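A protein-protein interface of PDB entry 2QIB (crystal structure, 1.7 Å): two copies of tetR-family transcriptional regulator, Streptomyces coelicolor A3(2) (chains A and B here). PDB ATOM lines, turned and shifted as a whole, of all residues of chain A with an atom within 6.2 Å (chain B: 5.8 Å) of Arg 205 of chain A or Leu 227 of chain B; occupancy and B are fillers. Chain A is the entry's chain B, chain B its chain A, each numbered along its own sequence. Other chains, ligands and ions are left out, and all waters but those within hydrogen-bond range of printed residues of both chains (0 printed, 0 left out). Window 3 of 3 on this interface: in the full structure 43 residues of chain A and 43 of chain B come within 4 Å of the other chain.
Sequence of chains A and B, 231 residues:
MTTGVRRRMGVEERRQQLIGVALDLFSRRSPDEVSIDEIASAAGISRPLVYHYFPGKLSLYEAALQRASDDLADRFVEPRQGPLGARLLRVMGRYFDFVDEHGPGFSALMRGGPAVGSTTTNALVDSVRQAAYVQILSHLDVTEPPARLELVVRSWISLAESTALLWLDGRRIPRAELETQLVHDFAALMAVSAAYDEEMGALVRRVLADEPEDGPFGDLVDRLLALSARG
Among the printed residues, pairs that only touch across the chains: Phe 217 of chain A with Ser 228 of chain B (3.2 Å), Ala 191 of chain A with Leu 224 of chain B (3.4 Å), Arg 205 of chain A with Leu 227 of chain B (3.5 Å), Gly 201 of chain A with Leu 227 of chain B (3.5 Å), Ala 194 of chain A with Leu 227 of chain B (3.6 Å) and Ala 195 of chain A with Leu 224 of chain B (3.9 Å).
No position is printed for both chains. Of the 7 pairs that touch across the chains among the printed residues, none has its exchanged pair printed and touching as well.
Printed residues of chain A that touch a printed residue of chain B: Ala 191, Ala 194, Ala 195, Gly 201, Arg 205 and Phe 217. Of the 8 printed residues of chain B, 4 touch a printed residue of chain A. Among the printed residues, no Asp or Glu carboxylate lies within 4 Å of a Lys or Arg side-chain nitrogen of the other chain.
O of Ala 195 of chain A lies within hydrogen-bond range of NH1 of Arg 223 of chain B, 3.1 Å away.
O of Leu 224 of chain B sits at hydrogen-bond distance from OG of Ser 228 of chain B. The guanidinium group (NH2) of Arg 205 of chain A is in salt-bridge range of the side-chain carboxylate (OE2) of Glu 198 of chain A.
Of chain B, only Leu 227 comes within 4 Å of Arg 205 of chain A. Leu 227 of chain B touches three residues of chain A. Of the printed residues of chain B, Phe 217 of chain A touches Ser 228 (3.2 Å). Printed residues of chain A within 4 Å of Leu 224 of chain B: Ala 191 (3.4 Å) and Ala 195 (3.9 Å). Of the printed residues of chain B, Ala 191 of chain A touches Leu 224 (3.4 Å). Printed residues of chain B within 4 Å of Ala 195 of chain A: Arg 223 and Leu 224. Printed residues of chain B within 4 Å of Gly 201 of chain A: Leu 227. Met 200 of chain A touches none of the printed residues of chain B. Ala 209 of chain A touches none of the printed residues of chain B. The nearest residue of chain A that does not touch Leu 227 of chain B is Val 204 of chain A (4.1 Å). The nearest printed residue of chain B that does not touch Gly 201 of chain A is Ser 228 of chain B (7.8 Å).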
ATOM      1  N   ALA A 191      27.147  24.270   4.266  1.00  0.00           N
ATOM      2  CA  ALA A 191      26.035  23.398   3.875  1.00  0.00           C
ATOM      3  C   ALA A 191      26.470  21.921   3.893  1.00  0.00           C
ATOM      4  O   ALA A 191      25.709  21.029   4.336  1.00  0.00           O
ATOM      5  CB  ALA A 191      25.571  23.787   2.490  1.00  0.00           C
ATOM      6  N   ALA A 194      26.599  20.844   7.489  1.00  0.00           N
ATOM      7  CA  ALA A 194      25.220  20.849   7.985  1.00  0.00           C
ATOM      8  C   ALA A 194      24.388  19.684   7.475  1.00  0.00           C
ATOM      9  O   ALA A 194      23.453  19.232   8.153  1.00  0.00           O
ATOM     10  CB  ALA A 194      24.554  22.198   7.638  1.00  0.00           C
ATOM     11  N   ALA A 195      24.728  19.167   6.297  1.00  0.00           N
ATOM     12  CA  ALA A 195      23.957  18.075   5.688  1.00  0.00           C
ATOM     13  C   ALA A 195      24.042  16.764   6.498  1.00  0.00           C
ATOM     14  O   ALA A 195      23.118  15.950   6.451  1.00  0.00           O
ATOM     15  CB  ALA A 195      24.424  17.845   4.226  1.00  0.00           C
ATOM     16  N   GLU A 198      23.590  17.362  12.947  1.00  0.00           N
ATOM     17  CA  GLU A 198      22.356  18.027  13.395  1.00  0.00           C
ATOM     18  C   GLU A 198      22.592  19.456  13.940  1.00  0.00           C
ATOM     19  O   GLU A 198      21.866  20.419  13.598  1.00  0.00           O
ATOM     20  CB  GLU A 198      21.621  17.128  14.412  1.00  0.00           C
ATOM     21  CG  GLU A 198      20.203  17.588  14.726  1.00  0.00           C
ATOM     22  CD  GLU A 198      19.437  18.040  13.490  1.00  0.00           C
ATOM     23  OE1 GLU A 198      19.069  17.174  12.670  1.00  0.00           O
ATOM     24  OE2 GLU A 198      19.208  19.265  13.341  1.00  0.00           O
ATOM     25  N   MET A 200      25.134  21.465  13.257  1.00  0.00           N
ATOM     26  CA  MET A 200      25.447  22.343  12.133  1.00  0.00           C
ATOM     27  C   MET A 200      24.180  22.625  11.329  1.00  0.00           C
ATOM     28  O   MET A 200      23.968  23.745  10.877  1.00  0.00           O
ATOM     29  CB  MET A 200      26.534  21.744  11.226  1.00  0.00           C
ATOM     30  CG  MET A 200      27.941  21.875  11.730  1.00  0.00           C
ATOM     31  SD  MET A 200      28.525  23.782  11.929  1.00  0.00           S
ATOM     32  CE  MET A 200      28.688  24.238  10.040  1.00  0.00           C
ATOM     33  N   GLY A 201      23.325  21.614  11.192  1.00  0.00           N
ATOM     34  CA  GLY A 201      22.047  21.816  10.492  1.00  0.00           C
ATOM     35  C   GLY A 201      21.209  22.897  11.175  1.00  0.00           C
ATOM     36  O   GLY A 201      20.656  23.786  10.516  1.00  0.00           O
ATOM     37  N   ALA A 202      21.146  22.842  12.508  1.00  0.00           N
ATOM     38  CA  ALA A 202      20.391  23.856  13.286  1.00  0.00           C
ATOM     39  C   ALA A 202      20.936  25.270  13.101  1.00  0.00           C
ATOM     40  O   ALA A 202      20.167  26.225  12.957  1.00  0.00           O
ATOM     41  CB  ALA A 202      20.348  23.479  14.773  1.00  0.00           C
ATOM     42  N   LEU A 203      22.265  25.405  13.106  1.00  0.00           N
ATOM     43  CA  LEU A 203      22.930  26.686  12.881  1.00  0.00           C
ATOM     44  C   LEU A 203      22.583  27.265  11.516  1.00  0.00           C
ATOM     45  O   LEU A 203      22.289  28.450  11.402  1.00  0.00           O
ATOM     46  CB  LEU A 203      24.458  26.524  13.005  1.00  0.00           C
ATOM     47  CG  LEU A 203      25.293  27.807  12.970  1.00  0.00           C
ATOM     48  CD1 LEU A 203      26.681  27.565  13.535  1.00  0.00           C
ATOM     49  CD2 LEU A 203      25.418  28.366  11.576  1.00  0.00           C
ATOM     50  N   VAL A 204      22.634  26.431  10.478  1.00  0.00           N
ATOM     51  CA  VAL A 204      22.329  26.879   9.123  1.00  0.00           C
ATOM     52  C   VAL A 204      20.881  27.368   9.023  1.00  0.00           C
ATOM     53  O   VAL A 204      20.640  28.446   8.475  1.00  0.00           O
ATOM     54  CB  VAL A 204      22.655  25.788   8.058  1.00  0.00           C
ATOM     55  CG1 VAL A 204      21.993  26.106   6.713  1.00  0.00           C
ATOM     56  CG2 VAL A 204      24.146  25.665   7.890  1.00  0.00           C
ATOM     57  N   ARG A 205      19.948  26.597   9.589  1.00  0.00           N
ATOM     58  CA  ARG A 205      18.517  26.955   9.621  1.00  0.00           C
ATOM     59  C   ARG A 205      18.250  28.262  10.376  1.00  0.00           C
ATOM     60  O   ARG A 205      17.375  29.042   9.992  1.00  0.00           O
ATOM     61  CB  ARG A 205      17.688  25.830  10.249  1.00  0.00           C
ATOM     62  CG  ARG A 205      17.524  24.572   9.396  1.00  0.00           C
ATOM     63  CD  ARG A 205      16.441  23.654   9.989  1.00  0.00           C
ATOM     64  NE  ARG A 205      16.814  23.186  11.327  1.00  0.00           N
ATOM     65  CZ  ARG A 205      17.249  21.958  11.611  1.00  0.00           C
ATOM     66  NH1 ARG A 205      17.340  21.038  10.660  1.00  0.00           N
ATOM     67  NH2 ARG A 205      17.579  21.643  12.855  1.00  0.00           N
ATOM     68  N   ARG A 206      18.984  28.470  11.466  1.00  0.00           N
ATOM     69  CA  ARG A 206      18.924  29.699  12.256  1.00  0.00           C
ATOM     70  C   ARG A 206      19.484  30.865  11.438  1.00  0.00           C
ATOM     71  O   ARG A 206      18.978  31.991  11.512  1.00  0.00           O
ATOM     72  CB  ARG A 206      19.706  29.488  13.561  1.00  0.00           C
ATOM     73  CG  ARG A 206      19.945  30.703  14.461  1.00  0.00           C
ATOM     74  CD  ARG A 206      20.768  30.285  15.694  1.00  0.00           C
ATOM     75  NE  ARG A 206      20.183  29.110  16.352  1.00  0.00           N
ATOM     76  CZ  ARG A 206      20.784  27.927  16.530  1.00  0.00           C
ATOM     77  NH1 ARG A 206      22.034  27.720  16.133  1.00  0.00           N
ATOM     78  NH2 ARG A 206      20.119  26.939  17.129  1.00  0.00           N
ATOM     79  N   VAL A 207      20.506  30.559  10.637  1.00  0.00           N
ATOM     80  CA  VAL A 207      21.230  31.523   9.805  1.00  0.00           C
ATOM     81  C   VAL A 207      20.601  31.732   8.415  1.00  0.00           C
ATOM     82  O   VAL A 207      20.942  32.692   7.724  1.00  0.00           O
ATOM     83  CB  VAL A 207      22.758  31.144   9.725  1.00  0.00           C
ATOM     84  CG1 VAL A 207      23.432  31.639   8.451  1.00  0.00           C
ATOM     85  CG2 VAL A 207      23.500  31.651  10.961  1.00  0.00           C
ATOM     86  N   LEU A 208      19.685  30.852   8.006  1.00  0.00           N
ATOM     87  CA  LEU A 208      18.953  31.049   6.739  1.00  0.00           C
ATOM     88  C   LEU A 208      17.606  31.760   6.927  1.00  0.00           C
ATOM     89  O   LEU A 208      16.932  32.104   5.951  1.00  0.00           O
ATOM     90  CB  LEU A 208      18.793  29.737   5.929  1.00  0.00           C
ATOM     91  CG  LEU A 208      17.967  28.503   6.358  1.00  0.00           C
ATOM     92  CD1 LEU A 208      16.502  28.811   6.712  1.00  0.00           C
ATOM     93  CD2 LEU A 208      18.024  27.406   5.297  1.00  0.00           C
ATOM     94  N   ALA A 209      17.227  31.971   8.187  1.00  0.00           N
ATOM     95  CA  ALA A 209      15.976  32.650   8.533  1.00  0.00           C
ATOM     96  C   ALA A 209      15.946  34.128   8.104  1.00  0.00           C
ATOM     97  O   ALA A 209      14.906  34.785   8.209  1.00  0.00           O
ATOM     98  CB  ALA A 209      15.704  32.518  10.028  1.00  0.00           C
ATOM     99  N   ASP A 210      17.076  34.639   7.613  1.00  0.00           N
ATOM    100  CA  ASP A 210      17.193  36.056   7.242  1.00  0.00           C
ATOM    101  C   ASP A 210      17.779  36.295   5.843  1.00  0.00           C
ATOM    102  O   ASP A 210      18.032  37.441   5.455  1.00  0.00           O
ATOM    103  CB  ASP A 210      17.986  36.828   8.307  1.00  0.00           C
ATOM    104  CG  ASP A 210      17.297  36.821   9.668  1.00  0.00           C
ATOM    105  OD1 ASP A 210      16.667  37.842  10.020  1.00  0.00           O
ATOM    106  OD2 ASP A 210      17.373  35.789  10.376  1.00  0.00           O
ATOM    107  N   PHE A 217      22.870  30.336   0.068  1.00  0.00           N
ATOM    108  CA  PHE A 217      22.518  28.947   0.381  1.00  0.00           C
ATOM    109  C   PHE A 217      21.441  28.409  -0.568  1.00  0.00           C
ATOM    110  O   PHE A 217      21.633  27.355  -1.187  1.00  0.00           O
ATOM    111  CB  PHE A 217      22.115  28.768   1.854  1.00  0.00           C
ATOM    112  CG  PHE A 217      21.741  27.345   2.218  1.00  0.00           C
ATOM    113  CD1 PHE A 217      22.722  26.365   2.381  1.00  0.00           C
ATOM    114  CD2 PHE A 217      20.403  26.986   2.390  1.00  0.00           C
ATOM    115  CE1 PHE A 217      22.373  25.047   2.715  1.00  0.00           C
ATOM    116  CE2 PHE A 217      20.042  25.675   2.727  1.00  0.00           C
ATOM    117  CZ  PHE A 217      21.029  24.704   2.888  1.00  0.00           C
ATOM    118  N   ASP B 222      19.761  15.467  -1.480  1.00  0.00           N
ATOM    119  CA  ASP B 222      18.548  15.062  -0.718  1.00  0.00           C
ATOM    120  C   ASP B 222      18.605  15.723   0.666  1.00  0.00           C
ATOM    121  O   ASP B 222      17.619  16.325   1.117  1.00  0.00           O
ATOM    122  CB  ASP B 222      18.471  13.543  -0.536  1.00  0.00           C
ATOM    123  CG  ASP B 222      18.188  12.785  -1.838  1.00  0.00           C
ATOM    124  OD1 ASP B 222      17.932  13.435  -2.865  1.00  0.00           O
ATOM    125  OD2 ASP B 222      18.241  11.533  -1.802  1.00  0.00           O
ATOM    126  N   ARG B 223      19.762  15.591   1.327  1.00  0.00           N
ATOM    127  CA  ARG B 223      19.957  16.193   2.662  1.00  0.00           C
ATOM    128  C   ARG B 223      19.858  17.715   2.711  1.00  0.00           C
ATOM    129  O   ARG B 223      19.324  18.302   3.671  1.00  0.00           O
ATOM    130  CB  ARG B 223      21.267  15.714   3.258  1.00  0.00           C
ATOM    131  CG  ARG B 223      21.198  14.266   3.684  1.00  0.00           C
ATOM    132  CD  ARG B 223      22.588  13.774   3.915  1.00  0.00           C
ATOM    133  NE  ARG B 223      22.576  12.389   4.362  1.00  0.00           N
ATOM    134  CZ  ARG B 223      22.631  12.014   5.635  1.00  0.00           C
ATOM    135  NH1 ARG B 223      22.674  12.926   6.608  1.00  0.00           N
ATOM    136  NH2 ARG B 223      22.632  10.717   5.930  1.00  0.00           N
ATOM    137  N   LEU B 224      20.358  18.378   1.667  1.00  0.00           N
ATOM    138  CA  LEU B 224      20.255  19.816   1.619  1.00  0.00           C
ATOM    139  C   LEU B 224      18.827  20.284   1.349  1.00  0.00           C
ATOM    140  O   LEU B 224      18.377  21.306   1.882  1.00  0.00           O
ATOM    141  CB  LEU B 224      21.234  20.389   0.584  1.00  0.00           C
ATOM    142  CG  LEU B 224      22.721  20.244   0.965  1.00  0.00           C
ATOM    143  CD1 LEU B 224      23.561  20.800  -0.168  1.00  0.00           C
ATOM    144  CD2 LEU B 224      23.023  20.982   2.279  1.00  0.00           C
ATOM    145  N   LEU B 225      18.105  19.520   0.532  1.00  0.00           N
ATOM    146  CA  LEU B 225      16.702  19.815   0.303  1.00  0.00           C
ATOM    147  C   LEU B 225      15.937  19.672   1.615  1.00  0.00           C
ATOM    148  O   LEU B 225      15.121  20.539   1.958  1.00  0.00           O
ATOM    149  CB  LEU B 225      16.130  18.919  -0.808  1.00  0.00           C
ATOM    150  CG  LEU B 225      16.595  19.329  -2.216  1.00  0.00           C
ATOM    151  CD1 LEU B 225      16.212  18.209  -3.239  1.00  0.00           C
ATOM    152  CD2 LEU B 225      16.030  20.711  -2.619  1.00  0.00           C
ATOM    153  N   ALA B 226      16.254  18.621   2.365  1.00  0.00           N
ATOM    154  CA  ALA B 226      15.612  18.340   3.671  1.00  0.00           C
ATOM    155  C   ALA B 226      15.908  19.447   4.687  1.00  0.00           C
ATOM    156  O   ALA B 226      15.011  19.961   5.357  1.00  0.00           O
ATOM    157  CB  ALA B 226      16.031  16.976   4.204  1.00  0.00           C
ATOM    158  N   LEU B 227      17.166  19.852   4.758  1.00  0.00           N
ATOM    159  CA  LEU B 227      17.555  20.975   5.594  1.00  0.00           C
ATOM    160  C   LEU B 227      16.770  22.245   5.253  1.00  0.00           C
ATOM    161  O   LEU B 227      16.301  22.950   6.157  1.00  0.00           O
ATOM    162  CB  LEU B 227      19.074  21.197   5.487  1.00  0.00           C
ATOM    163  CG  LEU B 227      19.724  22.146   6.483  1.00  0.00           C
ATOM    164  CD1 LEU B 227      19.390  21.727   7.924  1.00  0.00           C
ATOM    165  CD2 LEU B 227      21.209  22.089   6.227  1.00  0.00           C
ATOM    166  N   SER B 228      16.605  22.520   3.958  1.00  0.00           N
ATOM    167  CA  SER B 228      15.894  23.720   3.482  1.00  0.00           C
ATOM    168  C   SER B 228      14.395  23.669   3.779  1.00  0.00           C
ATOM    169  O   SER B 228      13.710  24.712   3.762  1.00  0.00           O
ATOM    170  CB  SER B 228      16.098  23.901   1.976  1.00  0.00           C
ATOM    171  OG  SER B 228      17.469  24.034   1.665  1.00  0.00           O
ATOM    172  N   ALA B 229      13.913  22.456   4.058  1.00  0.00           N
ATOM    173  CA  ALA B 229      12.492  22.181   4.314  1.00  0.00           C
ATOM    174  C   ALA B 229      11.620  22.803   3.228  1.00  0.00           C
ATOM    175  O   ALA B 229      10.672  23.538   3.505  1.00  0.00           O
ATOM    176  CB  ALA B 229      12.073  22.662   5.719  1.00  0.00           C
